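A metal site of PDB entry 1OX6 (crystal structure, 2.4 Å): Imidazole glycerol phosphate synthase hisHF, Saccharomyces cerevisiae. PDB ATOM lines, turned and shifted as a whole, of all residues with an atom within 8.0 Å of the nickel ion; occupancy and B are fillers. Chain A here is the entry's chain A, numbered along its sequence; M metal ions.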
ATOM      1  N   GLY A   1       0.880 -20.922  -0.866  1.00  0.00           N
ATOM      2  CA  GLY A   1       1.689 -21.929  -1.590  1.00  0.00           C
ATOM      3  C   GLY A   1       2.352 -21.384  -2.838  1.00  0.00           C
ATOM      4  O   GLY A   1       3.343 -21.918  -3.308  1.00  0.00           O
ATOM      5  N   SER A   2       1.803 -20.299  -3.366  1.00  0.00           N
ATOM      6  CA  SER A   2       2.340 -19.668  -4.565  1.00  0.00           C
ATOM      7  C   SER A   2       1.740 -18.281  -4.730  1.00  0.00           C
ATOM      8  O   SER A   2       1.960 -17.622  -5.741  1.00  0.00           O
ATOM      9  CB  SER A   2       2.010 -20.515  -5.783  1.00  0.00           C
ATOM     10  OG  SER A   2       0.608 -20.608  -5.970  1.00  0.00           O
ATOM     11  N   HIS A   3       0.978 -17.840  -3.741  1.00  0.00           N
ATOM     12  CA  HIS A   3       0.338 -16.532  -3.799  1.00  0.00           C
ATOM     13  C   HIS A   3       1.279 -15.423  -3.347  1.00  0.00           C
ATOM     14  O   HIS A   3       1.051 -14.255  -3.615  1.00  0.00           O
ATOM     15  CB  HIS A   3      -0.978 -16.537  -3.027  1.00  0.00           C
ATOM     16  CG  HIS A   3      -0.849 -16.650  -1.525  1.00  0.00           C
ATOM     17  ND1 HIS A   3      -0.105 -17.627  -0.911  1.00  0.00           N
ATOM     18  CD2 HIS A   3      -1.473 -15.973  -0.533  1.00  0.00           C
ATOM     19  CE1 HIS A   3      -0.277 -17.561   0.394  1.00  0.00           C
ATOM     20  NE2 HIS A   3      -1.113 -16.557   0.652  1.00  0.00           N
ATOM     21  N   MET A   4       2.318 -15.821  -2.634  1.00  0.00           N
ATOM     22  CA  MET A   4       3.364 -14.897  -2.213  1.00  0.00           C
ATOM     23  C   MET A   4       4.679 -15.687  -2.239  1.00  0.00           C
ATOM     24  O   MET A   4       4.682 -16.924  -2.145  1.00  0.00           O
ATOM     25  CB  MET A   4       3.080 -14.302  -0.839  1.00  0.00           C
ATOM     26  CG  MET A   4       2.951 -15.259   0.306  1.00  0.00           C
ATOM     27  SD  MET A   4       2.797 -14.294   1.802  1.00  0.00           S
ATOM     28  CE  MET A   4       1.079 -13.829   1.726  1.00  0.00           C
ATOM     29  N   PRO A   5       5.818 -14.996  -2.408  1.00  0.00           N
ATOM     30  CA  PRO A   5       7.087 -15.736  -2.432  1.00  0.00           C
ATOM     31  C   PRO A   5       7.357 -16.478  -1.135  1.00  0.00           C
ATOM     32  O   PRO A   5       7.249 -15.919  -0.044  1.00  0.00           O
ATOM     33  CB  PRO A   5       8.109 -14.663  -2.760  1.00  0.00           C
ATOM     34  CG  PRO A   5       7.514 -13.431  -2.174  1.00  0.00           C
ATOM     35  CD  PRO A   5       6.036 -13.543  -2.457  1.00  0.00           C
ATOM     36  N   VAL A   6       7.699 -17.752  -1.257  1.00  0.00           N
ATOM     37  CA  VAL A   6       7.953 -18.586  -0.095  1.00  0.00           C
ATOM     38  C   VAL A   6       9.434 -18.647   0.229  1.00  0.00           C
ATOM     39  O   VAL A   6      10.287 -18.733  -0.655  1.00  0.00           O
ATOM     40  CB  VAL A   6       7.441 -20.007  -0.309  1.00  0.00           C
ATOM     41  CG1 VAL A   6       7.655 -20.816   0.952  1.00  0.00           C
ATOM     42  CG2 VAL A   6       5.958 -19.990  -0.696  1.00  0.00           C
ATOM     43  N   GLU A  30       5.992 -15.743   2.706  1.00  0.00           N
ATOM     44  CA  GLU A  30       5.392 -16.866   3.387  1.00  0.00           C
ATOM     45  C   GLU A  30       6.527 -17.754   3.862  1.00  0.00           C
ATOM     46  O   GLU A  30       7.433 -18.090   3.094  1.00  0.00           O
ATOM     47  CB  GLU A  30       4.492 -17.655   2.439  1.00  0.00           C
ATOM     48  CG  GLU A  30       3.916 -18.909   3.061  1.00  0.00           C
ATOM     49  CD  GLU A  30       3.048 -19.668   2.106  1.00  0.00           C
ATOM     50  OE1 GLU A  30       2.122 -19.050   1.532  1.00  0.00           O
ATOM     51  OE2 GLU A  30       3.269 -20.875   1.914  1.00  0.00           O
HETATM   52 NI    NI M   1       0.748 -18.942  -2.078  1.00  0.00          NI
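SD of Met 4 sits at hydrogen-bond distance from N of Glu 30, at 3.6 Å. The backbone carbonyl oxygen (O) of Pro 5 is in hydrogen-bond range of the backbone NH (N) of Glu 30. N of Gly 1 sits close to OE1 of Glu 30, 3.3 Å away.
Merely in contact with the nickel ion: Met 4 (3.5 Å) and Glu 30 (3.9 Å). Within 4 Å of the nickel ion: Gly 1, Ser 2, His 3, Met 4 and Glu 30. Along chain A the residues within 4 Å of the nickel ion span positions 1 to 30. The nearest printed residue that does not touch the nickel ion is Val 6 (5.5 Å).
ND1 of His 3 binds the nickel ion (2.0 Å). The nickel ion is bound by N of His 3 (2.0 Å). The backbone nitrogen (N) of Ser 2 binds the nickel ion. The nickel ion is bound by N of Gly 1 (2.3 Å). The nickel ion has four donor atoms within binding distance.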
